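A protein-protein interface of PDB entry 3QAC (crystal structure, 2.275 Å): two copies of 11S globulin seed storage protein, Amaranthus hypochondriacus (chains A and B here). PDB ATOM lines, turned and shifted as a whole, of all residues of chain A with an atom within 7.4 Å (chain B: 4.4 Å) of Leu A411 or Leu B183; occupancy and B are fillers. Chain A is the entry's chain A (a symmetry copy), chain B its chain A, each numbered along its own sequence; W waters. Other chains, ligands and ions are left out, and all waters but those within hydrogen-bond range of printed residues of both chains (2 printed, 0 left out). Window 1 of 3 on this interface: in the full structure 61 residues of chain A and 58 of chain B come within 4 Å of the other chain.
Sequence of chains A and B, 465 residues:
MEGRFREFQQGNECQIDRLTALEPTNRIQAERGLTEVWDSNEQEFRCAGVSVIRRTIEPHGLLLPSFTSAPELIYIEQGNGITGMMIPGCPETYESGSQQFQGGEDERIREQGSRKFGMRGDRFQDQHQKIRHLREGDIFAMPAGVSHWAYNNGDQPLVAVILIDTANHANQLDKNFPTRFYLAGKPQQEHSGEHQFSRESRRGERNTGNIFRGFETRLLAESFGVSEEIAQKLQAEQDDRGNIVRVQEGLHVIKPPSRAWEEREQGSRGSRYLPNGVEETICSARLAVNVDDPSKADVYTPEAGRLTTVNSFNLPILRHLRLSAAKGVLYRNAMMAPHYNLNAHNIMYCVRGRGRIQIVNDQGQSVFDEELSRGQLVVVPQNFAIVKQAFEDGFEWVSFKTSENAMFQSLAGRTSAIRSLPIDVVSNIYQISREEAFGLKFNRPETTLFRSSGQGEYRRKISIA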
ATOM      1  N   ALA A 337     -28.940   0.595   8.330  1.00  0.00           N
ATOM      2  CA  ALA A 337     -27.693  -0.133   8.467  1.00  0.00           C
ATOM      3  C   ALA A 337     -27.229  -0.188   9.912  1.00  0.00           C
ATOM      4  O   ALA A 337     -27.531   0.699  10.707  1.00  0.00           O
ATOM      5  CB  ALA A 337     -26.617   0.481   7.609  1.00  0.00           C
ATOM      6  N   PRO A 338     -26.474  -1.236  10.249  1.00  0.00           N
ATOM      7  CA  PRO A 338     -25.906  -1.281  11.593  1.00  0.00           C
ATOM      8  C   PRO A 338     -25.189   0.037  11.844  1.00  0.00           C
ATOM      9  O   PRO A 338     -24.423   0.486  11.003  1.00  0.00           O
ATOM     10  CB  PRO A 338     -24.893  -2.424  11.503  1.00  0.00           C
ATOM     11  CG  PRO A 338     -25.394  -3.294  10.400  1.00  0.00           C
ATOM     12  CD  PRO A 338     -25.993  -2.338   9.402  1.00  0.00           C
ATOM     13  N   HIS A 339     -25.467   0.658  12.979  1.00  0.00           N
ATOM     14  CA  HIS A 339     -24.843   1.916  13.320  1.00  0.00           C
ATOM     15  C   HIS A 339     -24.734   1.984  14.822  1.00  0.00           C
ATOM     16  O   HIS A 339     -25.340   1.188  15.541  1.00  0.00           O
ATOM     17  CB  HIS A 339     -25.700   3.085  12.848  1.00  0.00           C
ATOM     18  CG  HIS A 339     -27.090   3.045  13.391  1.00  0.00           C
ATOM     19  ND1 HIS A 339     -28.019   2.121  12.969  1.00  0.00           N
ATOM     20  CD2 HIS A 339     -27.704   3.793  14.340  1.00  0.00           C
ATOM     21  CE1 HIS A 339     -29.150   2.307  13.626  1.00  0.00           C
ATOM     22  NE2 HIS A 339     -28.985   3.317  14.462  1.00  0.00           N
ATOM     23  N   TYR A 340     -23.951   2.942  15.294  1.00  0.00           N
ATOM     24  CA  TYR A 340     -23.887   3.205  16.706  1.00  0.00           C
ATOM     25  C   TYR A 340     -23.954   4.688  16.918  1.00  0.00           C
ATOM     26  O   TYR A 340     -23.508   5.458  16.088  1.00  0.00           O
ATOM     27  CB  TYR A 340     -22.609   2.636  17.287  1.00  0.00           C
ATOM     28  CG  TYR A 340     -21.354   3.416  16.961  1.00  0.00           C
ATOM     29  CD1 TYR A 340     -20.686   3.235  15.762  1.00  0.00           C
ATOM     30  CD2 TYR A 340     -20.830   4.300  17.875  1.00  0.00           C
ATOM     31  CE1 TYR A 340     -19.521   3.929  15.488  1.00  0.00           C
ATOM     32  CE2 TYR A 340     -19.678   4.987  17.624  1.00  0.00           C
ATOM     33  CZ  TYR A 340     -19.018   4.807  16.432  1.00  0.00           C
ATOM     34  OH  TYR A 340     -17.860   5.516  16.194  1.00  0.00           O
ATOM     35  N   ALA A 385     -23.886  -0.904  19.273  1.00  0.00           N
ATOM     36  CA  ALA A 385     -24.204  -1.043  17.862  1.00  0.00           C
ATOM     37  C   ALA A 385     -25.583  -1.642  17.654  1.00  0.00           C
ATOM     38  O   ALA A 385     -26.013  -2.532  18.397  1.00  0.00           O
ATOM     39  CB  ALA A 385     -23.165  -1.866  17.164  1.00  0.00           C
ATOM     40  N   ILE A 386     -26.272  -1.139  16.633  1.00  0.00           N
ATOM     41  CA  ILE A 386     -27.647  -1.513  16.381  1.00  0.00           C
ATOM     42  C   ILE A 386     -28.019  -1.485  14.891  1.00  0.00           C
ATOM     43  O   ILE A 386     -27.515  -0.653  14.135  1.00  0.00           O
ATOM     44  CB  ILE A 386     -28.626  -0.671  17.226  1.00  0.00           C
ATOM     45  CG1 ILE A 386     -30.054  -0.866  16.741  1.00  0.00           C
ATOM     46  CG2 ILE A 386     -28.249   0.819  17.195  1.00  0.00           C
ATOM     47  CD1 ILE A 386     -31.064  -0.153  17.562  1.00  0.00           C
ATOM     48  N   VAL A 387     -28.861  -2.441  14.490  1.00  0.00           N
ATOM     49  CA  VAL A 387     -29.467  -2.506  13.158  1.00  0.00           C
ATOM     50  C   VAL A 387     -30.986  -2.635  13.297  1.00  0.00           C
ATOM     51  O   VAL A 387     -31.498  -3.238  14.238  1.00  0.00           O
ATOM     52  CB  VAL A 387     -28.896  -3.678  12.314  1.00  0.00           C
ATOM     53  CG1 VAL A 387     -29.119  -5.022  13.012  1.00  0.00           C
ATOM     54  CG2 VAL A 387     -29.486  -3.669  10.900  1.00  0.00           C
ATOM     55  N   PHE A 408     -24.785   9.794  15.101  1.00  0.00           N
ATOM     56  CA  PHE A 408     -24.531   8.378  15.001  1.00  0.00           C
ATOM     57  C   PHE A 408     -23.614   8.112  13.838  1.00  0.00           C
ATOM     58  O   PHE A 408     -23.352   9.002  13.047  1.00  0.00           O
ATOM     59  CB  PHE A 408     -25.826   7.582  14.876  1.00  0.00           C
ATOM     60  CG  PHE A 408     -26.534   7.770  13.572  1.00  0.00           C
ATOM     61  CD1 PHE A 408     -26.134   7.079  12.446  1.00  0.00           C
ATOM     62  CD2 PHE A 408     -27.618   8.613  13.478  1.00  0.00           C
ATOM     63  CE1 PHE A 408     -26.806   7.237  11.243  1.00  0.00           C
ATOM     64  CE2 PHE A 408     -28.288   8.783  12.269  1.00  0.00           C
ATOM     65  CZ  PHE A 408     -27.887   8.089  11.161  1.00  0.00           C
ATOM     66  N   GLN A 409     -23.109   6.890  13.749  1.00  0.00           N
ATOM     67  CA  GLN A 409     -22.286   6.508  12.627  1.00  0.00           C
ATOM     68  C   GLN A 409     -22.769   5.191  12.086  1.00  0.00           C
ATOM     69  O   GLN A 409     -22.806   4.188  12.806  1.00  0.00           O
ATOM     70  CB  GLN A 409     -20.814   6.382  13.025  1.00  0.00           C
ATOM     71  CG  GLN A 409     -20.013   5.558  12.019  1.00  0.00           C
ATOM     72  CD  GLN A 409     -18.532   5.915  11.984  1.00  0.00           C
ATOM     73  OE1 GLN A 409     -18.133   6.866  11.319  1.00  0.00           O
ATOM     74  NE2 GLN A 409     -17.713   5.139  12.685  1.00  0.00           N
ATOM     75  N   SER A 410     -23.145   5.193  10.818  1.00  0.00           N
ATOM     76  CA  SER A 410     -23.437   3.956  10.124  1.00  0.00           C
ATOM     77  C   SER A 410     -22.152   3.166   9.969  1.00  0.00           C
ATOM     78  O   SER A 410     -21.069   3.726   9.871  1.00  0.00           O
ATOM     79  CB  SER A 410     -24.047   4.242   8.756  1.00  0.00           C
ATOM     80  OG  SER A 410     -25.191   5.063   8.900  1.00  0.00           O
ATOM     81  N   LEU A 411     -22.268   1.856   9.950  1.00  0.00           N
ATOM     82  CA  LEU A 411     -21.103   1.025   9.752  1.00  0.00           C
ATOM     83  C   LEU A 411     -21.016   0.656   8.282  1.00  0.00           C
ATOM     84  O   LEU A 411     -19.928   0.503   7.741  1.00  0.00           O
ATOM     85  CB  LEU A 411     -21.210  -0.211  10.624  1.00  0.00           C
ATOM     86  CG  LEU A 411     -21.456   0.191  12.080  1.00  0.00           C
ATOM     87  CD1 LEU A 411     -21.922  -1.002  12.920  1.00  0.00           C
ATOM     88  CD2 LEU A 411     -20.200   0.823  12.664  1.00  0.00           C
ATOM     89  N   ALA A 412     -22.175   0.543   7.635  1.00  0.00           N
ATOM     90  CA  ALA A 412     -22.245   0.223   6.209  1.00  0.00           C
ATOM     91  C   ALA A 412     -22.794   1.386   5.395  1.00  0.00           C
ATOM     92  O   ALA A 412     -23.524   2.225   5.912  1.00  0.00           O
ATOM     93  CB  ALA A 412     -23.097  -1.029   5.983  1.00  0.00           C
ATOM     94  N   GLY A 413     -22.436   1.435   4.116  1.00  0.00           N
ATOM     95  CA  GLY A 413     -23.046   2.381   3.194  1.00  0.00           C
ATOM     96  C   GLY A 413     -22.244   3.633   2.917  1.00  0.00           C
ATOM     97  O   GLY A 413     -21.081   3.745   3.296  1.00  0.00           O
ATOM     98  N   THR A 415     -21.027   7.261   3.556  1.00  0.00           N
ATOM     99  CA  THR A 415     -20.869   7.901   4.856  1.00  0.00           C
ATOM    100  C   THR A 415     -21.041   6.847   5.936  1.00  0.00           C
ATOM    101  O   THR A 415     -21.979   6.925   6.719  1.00  0.00           O
ATOM    102  CB  THR A 415     -21.934   8.993   5.076  1.00  0.00           C
ATOM    103  OG1 THR A 415     -21.909   9.909   3.975  1.00  0.00           O
ATOM    104  CG2 THR A 415     -21.661   9.747   6.367  1.00  0.00           C
ATOM    105  N   SER A 416     -20.158   5.847   5.940  1.00  0.00           N
ATOM    106  CA  SER A 416     -20.143   4.787   6.949  1.00  0.00           C
ATOM    107  C   SER A 416     -18.721   4.621   7.472  1.00  0.00           C
ATOM    108  O   SER A 416     -17.765   5.147   6.880  1.00  0.00           O
ATOM    109  CB  SER A 416     -20.613   3.460   6.353  1.00  0.00           C
ATOM    110  OG  SER A 416     -19.615   2.897   5.510  1.00  0.00           O
ATOM    111  N   ALA A 417     -18.575   3.897   8.577  1.00  0.00           N
ATOM    112  CA  ALA A 417     -17.252   3.671   9.126  1.00  0.00           C
ATOM    113  C   ALA A 417     -16.424   2.941   8.086  1.00  0.00           C
ATOM    114  O   ALA A 417     -15.315   3.346   7.781  1.00  0.00           O
ATOM    115  CB  ALA A 417     -17.327   2.873  10.380  1.00  0.00           C
ATOM    116  N   ILE A 418     -16.978   1.871   7.534  1.00  0.00           N
ATOM    117  CA  ILE A 418     -16.244   1.048   6.579  1.00  0.00           C
ATOM    118  C   ILE A 418     -15.774   1.864   5.373  1.00  0.00           C
ATOM    119  O   ILE A 418     -14.609   1.813   4.986  1.00  0.00           O
ATOM    120  CB  ILE A 418     -17.102  -0.139   6.105  1.00  0.00           C
ATOM    121  CG1 ILE A 418     -17.428  -1.062   7.286  1.00  0.00           C
ATOM    122  CG2 ILE A 418     -16.408  -0.898   5.013  1.00  0.00           C
ATOM    123  CD1 ILE A 418     -16.225  -1.474   8.120  1.00  0.00           C
ATOM    124  N   ARG A 419     -16.690   2.618   4.779  1.00  0.00           N
ATOM    125  CA  ARG A 419     -16.359   3.402   3.598  1.00  0.00           C
ATOM    126  C   ARG A 419     -15.327   4.495   3.881  1.00  0.00           C
ATOM    127  O   ARG A 419     -14.556   4.861   3.009  1.00  0.00           O
ATOM    128  CB  ARG A 419     -17.614   4.017   3.012  1.00  0.00           C
ATOM    129  CG  ARG A 419     -17.347   4.787   1.764  1.00  0.00           C
ATOM    130  CD  ARG A 419     -18.481   4.603   0.791  1.00  0.00           C
ATOM    131  NE  ARG A 419     -18.524   5.704  -0.158  1.00  0.00           N
ATOM    132  CZ  ARG A 419     -19.336   5.739  -1.204  1.00  0.00           C
ATOM    133  NH1 ARG A 419     -19.314   6.795  -2.020  1.00  0.00           N
ATOM    134  NH2 ARG A 419     -20.168   4.715  -1.427  1.00  0.00           N
ATOM    135  N   SER A 420     -15.316   5.007   5.106  1.00  0.00           N
ATOM    136  CA  SER A 420     -14.305   5.970   5.518  1.00  0.00           C
ATOM    137  C   SER A 420     -12.917   5.341   5.682  1.00  0.00           C
ATOM    138  O   SER A 420     -11.912   6.050   5.702  1.00  0.00           O
ATOM    139  CB  SER A 420     -14.726   6.669   6.810  1.00  0.00           C
ATOM    140  OG  SER A 420     -15.878   7.467   6.595  1.00  0.00           O
ATOM    141  N   LEU A 421     -12.864   4.018   5.795  1.00  0.00           N
ATOM    142  CA  LEU A 421     -11.588   3.303   5.917  1.00  0.00           C
ATOM    143  C   LEU A 421     -10.846   3.179   4.588  1.00  0.00           C
ATOM    144  O   LEU A 421     -11.438   2.806   3.583  1.00  0.00           O
ATOM    145  CB  LEU A 421     -11.809   1.898   6.475  1.00  0.00           C
ATOM    146  CG  LEU A 421     -12.338   1.795   7.894  1.00  0.00           C
ATOM    147  CD1 LEU A 421     -12.554   0.355   8.254  1.00  0.00           C
ATOM    148  CD2 LEU A 421     -11.351   2.471   8.860  1.00  0.00           C
ATOM    149  N   ILE A 429      -7.446  -5.459   7.960  1.00  0.00           N
ATOM    150  CA  ILE A 429      -8.101  -5.719   9.246  1.00  0.00           C
ATOM    151  C   ILE A 429      -9.092  -6.856   9.145  1.00  0.00           C
ATOM    152  O   ILE A 429      -9.419  -7.491  10.147  1.00  0.00           O
ATOM    153  CB  ILE A 429      -8.845  -4.488   9.835  1.00  0.00           C
ATOM    154  CG1 ILE A 429      -9.956  -4.018   8.890  1.00  0.00           C
ATOM    155  CG2 ILE A 429      -7.876  -3.370  10.174  1.00  0.00           C
ATOM    156  CD1 ILE A 429     -10.719  -2.828   9.400  1.00  0.00           C
ATOM    157  N   TYR A 430      -9.585  -7.110   7.941  1.00  0.00           N
ATOM    158  CA  TYR A 430     -10.550  -8.180   7.779  1.00  0.00           C
ATOM    159  C   TYR A 430      -9.919  -9.405   7.136  1.00  0.00           C
ATOM    160  O   TYR A 430     -10.563 -10.439   7.001  1.00  0.00           O
ATOM    161  CB  TYR A 430     -11.775  -7.686   7.008  1.00  0.00           C
ATOM    162  CG  TYR A 430     -12.547  -6.648   7.788  1.00  0.00           C
ATOM    163  CD1 TYR A 430     -12.750  -5.368   7.275  1.00  0.00           C
ATOM    164  CD2 TYR A 430     -13.032  -6.930   9.069  1.00  0.00           C
ATOM    165  CE1 TYR A 430     -13.447  -4.407   7.989  1.00  0.00           C
ATOM    166  CE2 TYR A 430     -13.728  -5.976   9.801  1.00  0.00           C
ATOM    167  CZ  TYR A 430     -13.935  -4.708   9.254  1.00  0.00           C
ATOM    168  OH  TYR A 430     -14.623  -3.732   9.965  1.00  0.00           O
ATOM    169  N   LEU A 440     -16.929  -4.741  -0.009  1.00  0.00           N
ATOM    170  CA  LEU A 440     -17.319  -4.455   1.359  1.00  0.00           C
ATOM    171  C   LEU A 440     -17.556  -2.951   1.490  1.00  0.00           C
ATOM    172  O   LEU A 440     -18.524  -2.520   2.116  1.00  0.00           O
ATOM    173  CB  LEU A 440     -16.240  -4.914   2.336  1.00  0.00           C
ATOM    174  CG  LEU A 440     -16.550  -4.694   3.817  1.00  0.00           C
ATOM    175  CD1 LEU A 440     -17.905  -5.291   4.155  1.00  0.00           C
ATOM    176  CD2 LEU A 440     -15.452  -5.292   4.693  1.00  0.00           C
ATOM    177  N   LYS A 441     -16.682  -2.157   0.876  1.00  0.00           N
ATOM    178  CA  LYS A 441     -16.796  -0.709   0.959  1.00  0.00           C
ATOM    179  C   LYS A 441     -17.931  -0.137   0.121  1.00  0.00           C
ATOM    180  O   LYS A 441     -18.649   0.747   0.585  1.00  0.00           O
ATOM    181  CB  LYS A 441     -15.486  -0.018   0.575  1.00  0.00           C
ATOM    182  CG  LYS A 441     -14.369  -0.210   1.582  1.00  0.00           C
ATOM    183  CD  LYS A 441     -13.188   0.715   1.303  1.00  0.00           C
ATOM    184  CE  LYS A 441     -13.581   2.179   1.385  1.00  0.00           C
ATOM    185  NZ  LYS A 441     -12.390   3.069   1.261  1.00  0.00           N
ATOM    186  N   PHE A 450     -31.571   1.608   3.792  1.00  0.00           N
ATOM    187  CA  PHE A 450     -31.444   0.726   2.637  1.00  0.00           C
ATOM    188  C   PHE A 450     -32.760   0.048   2.338  1.00  0.00           C
ATOM    189  O   PHE A 450     -33.531  -0.259   3.242  1.00  0.00           O
ATOM    190  CB  PHE A 450     -30.453  -0.399   2.920  1.00  0.00           C
ATOM    191  CG  PHE A 450     -29.112   0.066   3.369  1.00  0.00           C
ATOM    192  CD1 PHE A 450     -28.267  -0.801   4.040  1.00  0.00           C
ATOM    193  CD2 PHE A 450     -28.688   1.364   3.120  1.00  0.00           C
ATOM    194  CE1 PHE A 450     -27.019  -0.384   4.450  1.00  0.00           C
ATOM    195  CE2 PHE A 450     -27.449   1.798   3.538  1.00  0.00           C
ATOM    196  CZ  PHE A 450     -26.606   0.928   4.201  1.00  0.00           C
ATOM    197  N   PRO B  65      -9.535  -0.568  13.967  1.00  0.00           N
ATOM    198  CA  PRO B  65     -10.482   0.478  14.332  1.00  0.00           C
ATOM    199  C   PRO B  65     -11.277   0.127  15.587  1.00  0.00           C
ATOM    200  O   PRO B  65     -11.778  -0.994  15.738  1.00  0.00           O
ATOM    201  CB  PRO B  65     -11.418   0.536  13.122  1.00  0.00           C
ATOM    202  CG  PRO B  65     -11.118  -0.705  12.321  1.00  0.00           C
ATOM    203  CD  PRO B  65      -9.667  -0.935  12.551  1.00  0.00           C
ATOM    204  N   PHE B  67     -13.724   2.348  18.967  1.00  0.00           N
ATOM    205  CA  PHE B  67     -14.114   3.580  19.625  1.00  0.00           C
ATOM    206  C   PHE B  67     -14.369   3.297  21.099  1.00  0.00           C
ATOM    207  O   PHE B  67     -14.532   2.161  21.494  1.00  0.00           O
ATOM    208  CB  PHE B  67     -15.338   4.208  18.958  1.00  0.00           C
ATOM    209  CG  PHE B  67     -16.481   3.244  18.718  1.00  0.00           C
ATOM    210  CD1 PHE B  67     -16.497   2.418  17.597  1.00  0.00           C
ATOM    211  CD2 PHE B  67     -17.553   3.186  19.596  1.00  0.00           C
ATOM    212  CE1 PHE B  67     -17.556   1.561  17.362  1.00  0.00           C
ATOM    213  CE2 PHE B  67     -18.619   2.321  19.366  1.00  0.00           C
ATOM    214  CZ  PHE B  67     -18.620   1.514  18.247  1.00  0.00           C
ATOM    215  N   MET B  86     -12.716   8.341  11.729  1.00  0.00           N
ATOM    216  CA  MET B  86     -13.921   8.263  10.915  1.00  0.00           C
ATOM    217  C   MET B  86     -15.017   9.063  11.567  1.00  0.00           C
ATOM    218  O   MET B  86     -15.915   8.507  12.202  1.00  0.00           O
ATOM    219  CB  MET B  86     -14.388   6.819  10.715  1.00  0.00           C
ATOM    220  CG  MET B  86     -13.407   5.947   9.937  1.00  0.00           C
ATOM    221  SD  MET B  86     -12.285   5.090  11.046  1.00  0.00           S
ATOM    222  CE  MET B  86     -13.314   3.714  11.566  1.00  0.00           C
ATOM    223  N   SER B 147     -14.732   6.618  16.096  1.00  0.00           N
ATOM    224  CA  SER B 147     -14.026   5.423  15.694  1.00  0.00           C
ATOM    225  C   SER B 147     -12.695   5.822  15.065  1.00  0.00           C
ATOM    226  O   SER B 147     -12.589   6.850  14.385  1.00  0.00           O
ATOM    227  CB  SER B 147     -14.869   4.655  14.690  1.00  0.00           C
ATOM    228  OG  SER B 147     -15.136   5.485  13.572  1.00  0.00           O
ATOM    229  N   PHE B 181     -15.233  -0.520  22.061  1.00  0.00           N
ATOM    230  CA  PHE B 181     -15.878  -1.286  21.009  1.00  0.00           C
ATOM    231  C   PHE B 181     -14.925  -1.350  19.816  1.00  0.00           C
ATOM    232  O   PHE B 181     -14.462  -0.317  19.341  1.00  0.00           O
ATOM    233  CB  PHE B 181     -17.179  -0.605  20.567  1.00  0.00           C
ATOM    234  CG  PHE B 181     -18.162  -0.330  21.684  1.00  0.00           C
ATOM    235  CD1 PHE B 181     -19.362  -1.016  21.752  1.00  0.00           C
ATOM    236  CD2 PHE B 181     -17.902   0.638  22.639  1.00  0.00           C
ATOM    237  CE1 PHE B 181     -20.285  -0.756  22.755  1.00  0.00           C
ATOM    238  CE2 PHE B 181     -18.819   0.907  23.644  1.00  0.00           C
ATOM    239  CZ  PHE B 181     -20.019   0.209  23.699  1.00  0.00           C
ATOM    240  N   TYR B 182     -14.618  -2.557  19.349  1.00  0.00           N
ATOM    241  CA  TYR B 182     -13.777  -2.726  18.161  1.00  0.00           C
ATOM    242  C   TYR B 182     -14.609  -3.043  16.930  1.00  0.00           C
ATOM    243  O   TYR B 182     -15.702  -3.622  17.018  1.00  0.00           O
ATOM    244  CB  TYR B 182     -12.723  -3.819  18.358  1.00  0.00           C
ATOM    245  CG  TYR B 182     -11.482  -3.356  19.080  1.00  0.00           C
ATOM    246  CD1 TYR B 182     -11.414  -3.360  20.461  1.00  0.00           C
ATOM    247  CD2 TYR B 182     -10.389  -2.902  18.381  1.00  0.00           C
ATOM    248  CE1 TYR B 182     -10.272  -2.938  21.126  1.00  0.00           C
ATOM    249  CE2 TYR B 182      -9.249  -2.471  19.030  1.00  0.00           C
ATOM    250  CZ  TYR B 182      -9.186  -2.496  20.403  1.00  0.00           C
ATOM    251  OH  TYR B 182      -8.037  -2.061  21.047  1.00  0.00           O
ATOM    252  N   LEU B 183     -14.067  -2.656  15.781  1.00  0.00           N
ATOM    253  CA  LEU B 183     -14.769  -2.771  14.515  1.00  0.00           C
ATOM    254  C   LEU B 183     -14.203  -3.893  13.669  1.00  0.00           C
ATOM    255  O   LEU B 183     -14.616  -4.086  12.531  1.00  0.00           O
ATOM    256  CB  LEU B 183     -14.666  -1.448  13.769  1.00  0.00           C
ATOM    257  CG  LEU B 183     -15.658  -0.456  14.349  1.00  0.00           C
ATOM    258  CD1 LEU B 183     -15.369   0.956  13.879  1.00  0.00           C
ATOM    259  CD2 LEU B 183     -17.049  -0.906  13.939  1.00  0.00           C
ATOM    260  N   ALA B 184     -13.248  -4.619  14.231  1.00  0.00           N
ATOM    261  CA  ALA B 184     -12.589  -5.706  13.526  1.00  0.00           C
ATOM    262  C   ALA B 184     -11.794  -6.554  14.513  1.00  0.00           C
ATOM    263  O   ALA B 184     -11.463  -6.101  15.607  1.00  0.00           O
ATOM    264  CB  ALA B 184     -11.658  -5.147  12.424  1.00  0.00           C
ATOM    265  N   ASN B 210     -15.365  -8.344  18.302  1.00  0.00           N
ATOM    266  CA  ASN B 210     -15.664  -7.007  17.784  1.00  0.00           C
ATOM    267  C   ASN B 210     -17.166  -6.871  17.551  1.00  0.00           C
ATOM    268  O   ASN B 210     -17.880  -7.871  17.539  1.00  0.00           O
ATOM    269  CB  ASN B 210     -14.881  -6.725  16.490  1.00  0.00           C
ATOM    270  CG  ASN B 210     -15.496  -7.405  15.269  1.00  0.00           C
ATOM    271  OD1 ASN B 210     -16.619  -7.101  14.881  1.00  0.00           O
ATOM    272  ND2 ASN B 210     -14.751  -8.316  14.651  1.00  0.00           N
ATOM    273  N   ILE B 211     -17.655  -5.649  17.370  1.00  0.00           N
ATOM    274  CA  ILE B 211     -19.102  -5.456  17.398  1.00  0.00           C
ATOM    275  C   ILE B 211     -19.827  -6.261  16.331  1.00  0.00           C
ATOM    276  O   ILE B 211     -20.980  -6.643  16.517  1.00  0.00           O
ATOM    277  CB  ILE B 211     -19.524  -3.979  17.297  1.00  0.00           C
ATOM    278  CG1 ILE B 211     -19.220  -3.418  15.914  1.00  0.00           C
ATOM    279  CG2 ILE B 211     -18.868  -3.163  18.387  1.00  0.00           C
ATOM    280  CD1 ILE B 211     -19.704  -2.012  15.766  1.00  0.00           C
ATOM    281  N   PHE B 212     -19.150  -6.517  15.215  1.00  0.00           N
ATOM    282  CA  PHE B 212     -19.765  -7.261  14.126  1.00  0.00           C
ATOM    283  C   PHE B 212     -20.076  -8.685  14.551  1.00  0.00           C
ATOM    284  O   PHE B 212     -21.113  -9.224  14.176  1.00  0.00           O
ATOM    285  CB  PHE B 212     -18.885  -7.239  12.880  1.00  0.00           C
ATOM    286  CG  PHE B 212     -18.801  -5.891  12.233  1.00  0.00           C
ATOM    287  CD1 PHE B 212     -17.583  -5.271  12.046  1.00  0.00           C
ATOM    288  CD2 PHE B 212     -19.952  -5.229  11.844  1.00  0.00           C
ATOM    289  CE1 PHE B 212     -17.509  -4.019  11.457  1.00  0.00           C
ATOM    290  CE2 PHE B 212     -19.887  -3.984  11.266  1.00  0.00           C
ATOM    291  CZ  PHE B 212     -18.661  -3.376  11.071  1.00  0.00           C
ATOM    292  N   PHE B 224     -24.084  -4.975   4.022  1.00  0.00           N
ATOM    293  CA  PHE B 224     -22.985  -4.490   3.201  1.00  0.00           C
ATOM    294  C   PHE B 224     -23.110  -4.847   1.722  1.00  0.00           C
ATOM    295  O   PHE B 224     -22.240  -4.499   0.932  1.00  0.00           O
ATOM    296  CB  PHE B 224     -21.645  -4.997   3.754  1.00  0.00           C
ATOM    297  CG  PHE B 224     -21.251  -4.365   5.066  1.00  0.00           C
ATOM    298  CD1 PHE B 224     -21.701  -4.888   6.266  1.00  0.00           C
ATOM    299  CD2 PHE B 224     -20.437  -3.237   5.092  1.00  0.00           C
ATOM    300  CE1 PHE B 224     -21.343  -4.307   7.464  1.00  0.00           C
ATOM    301  CE2 PHE B 224     -20.078  -2.649   6.294  1.00  0.00           C
ATOM    302  CZ  PHE B 224     -20.530  -3.184   7.480  1.00  0.00           C
HETATM  303  O   HOH W   1     -21.019  -2.195   1.213  1.00  0.00           O
HETATM  304  O   HOH W   2     -17.125   7.728  14.549  1.00  0.00           O
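Water W1 bridges O of Phe B224 and O of Leu A440.
Water W2 lies within hydrogen-bond range of the backbone carbonyl oxygen (O) of Met B86, the side-chain hydroxyl (OH) of Tyr A340, the backbone NH (N) of Ser B147 and the side-chain amide nitrogen (NE2) of Gln A409.
The backbone carbonyl oxygen of Pro A338 sits at hydrogen-bond distance from the backbone NH of Leu A411.
The backbone NH of Ile A418 sits close to the backbone carbonyl oxygen of Leu A411, 3.3 Å away.
Among the printed residues, merely in contact across the chains: Ile A418 with Phe B224 (3.2 Å), Tyr A430 with Phe B212 (3.3 Å), Tyr A340 with Phe B67 (3.3 Å), Leu A440 with Phe B224 (3.4 Å), Ala A412 with Phe B224 (3.4 Å), Tyr A430 with Ala B184 (3.4 Å), Ser A420 with Met B86 (3.5 Å), Leu A411 with Phe B224 (3.5 Å), Leu A421 with Met B86 (3.5 Å), Ile A429 with Pro B65 (3.6 Å), Ala A385 with Ile B211 (3.7 Å), Leu A411 with Ile B211 (3.7 Å), Leu A411 with Leu B183 (3.8 Å), Ile A429 with Ala B184 (3.9 Å), Ala A417 with Met B86 (3.9 Å) and Leu A411 with Phe B212 (3.97 Å).
Hydrophobic or aromatic side chains of chain B within 4 Å of the printed part of chain A: Pro B65, Phe B67, Met B86, Leu B183, Ala B184, Ile B211, Phe B212 and Phe B224.
Printed residues of chain A that touch a printed residue of chain B: Tyr A340, Ala A385, Gln A409, Leu A411, Ala A412, Ala A417, Ile A418, Ser A420, Leu A421, Ile A429, Tyr A430 and Leu A440.
Along chain A the printed residues that touch a printed residue of chain B span positions 340 to 440.
Leu A411 touches just these residues of chain B: Leu B183, Ile B211, Phe B212 and Phe B224.
Of the printed residues of chain B, Leu A421 touches Met B86.
Of the printed residues of chain A, Ser B147 touches Tyr A340 (3.3 Å) and Gln A409 (2.7 Å).
Leu B183 touches two residues of chain A.
Of the printed residues of chain A, Phe B212 touches Leu A411 (3.97 Å) and Tyr A430 (3.3 Å).
The nearest printed residue of chain A that does not touch Pro B65 is Leu A421 (4.4 Å).
No position is printed for both chains.
Of the 20 pairs that touch across the chains among the printed residues, none has its exchanged pair printed and touching as well.
OE1 of Gln A409 sits close to O of Met B86 (2.9 Å).
N of Ser B147 is in hydrogen-bond range of OH of Tyr A340, 3.3 Å away.
The side-chain hydroxyl (OG) of Ser B147 lies within hydrogen-bond range of the side-chain amide nitrogen (NE2) of Gln A409.
O of Leu B183 lies within hydrogen-bond range of OH of Tyr A430.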
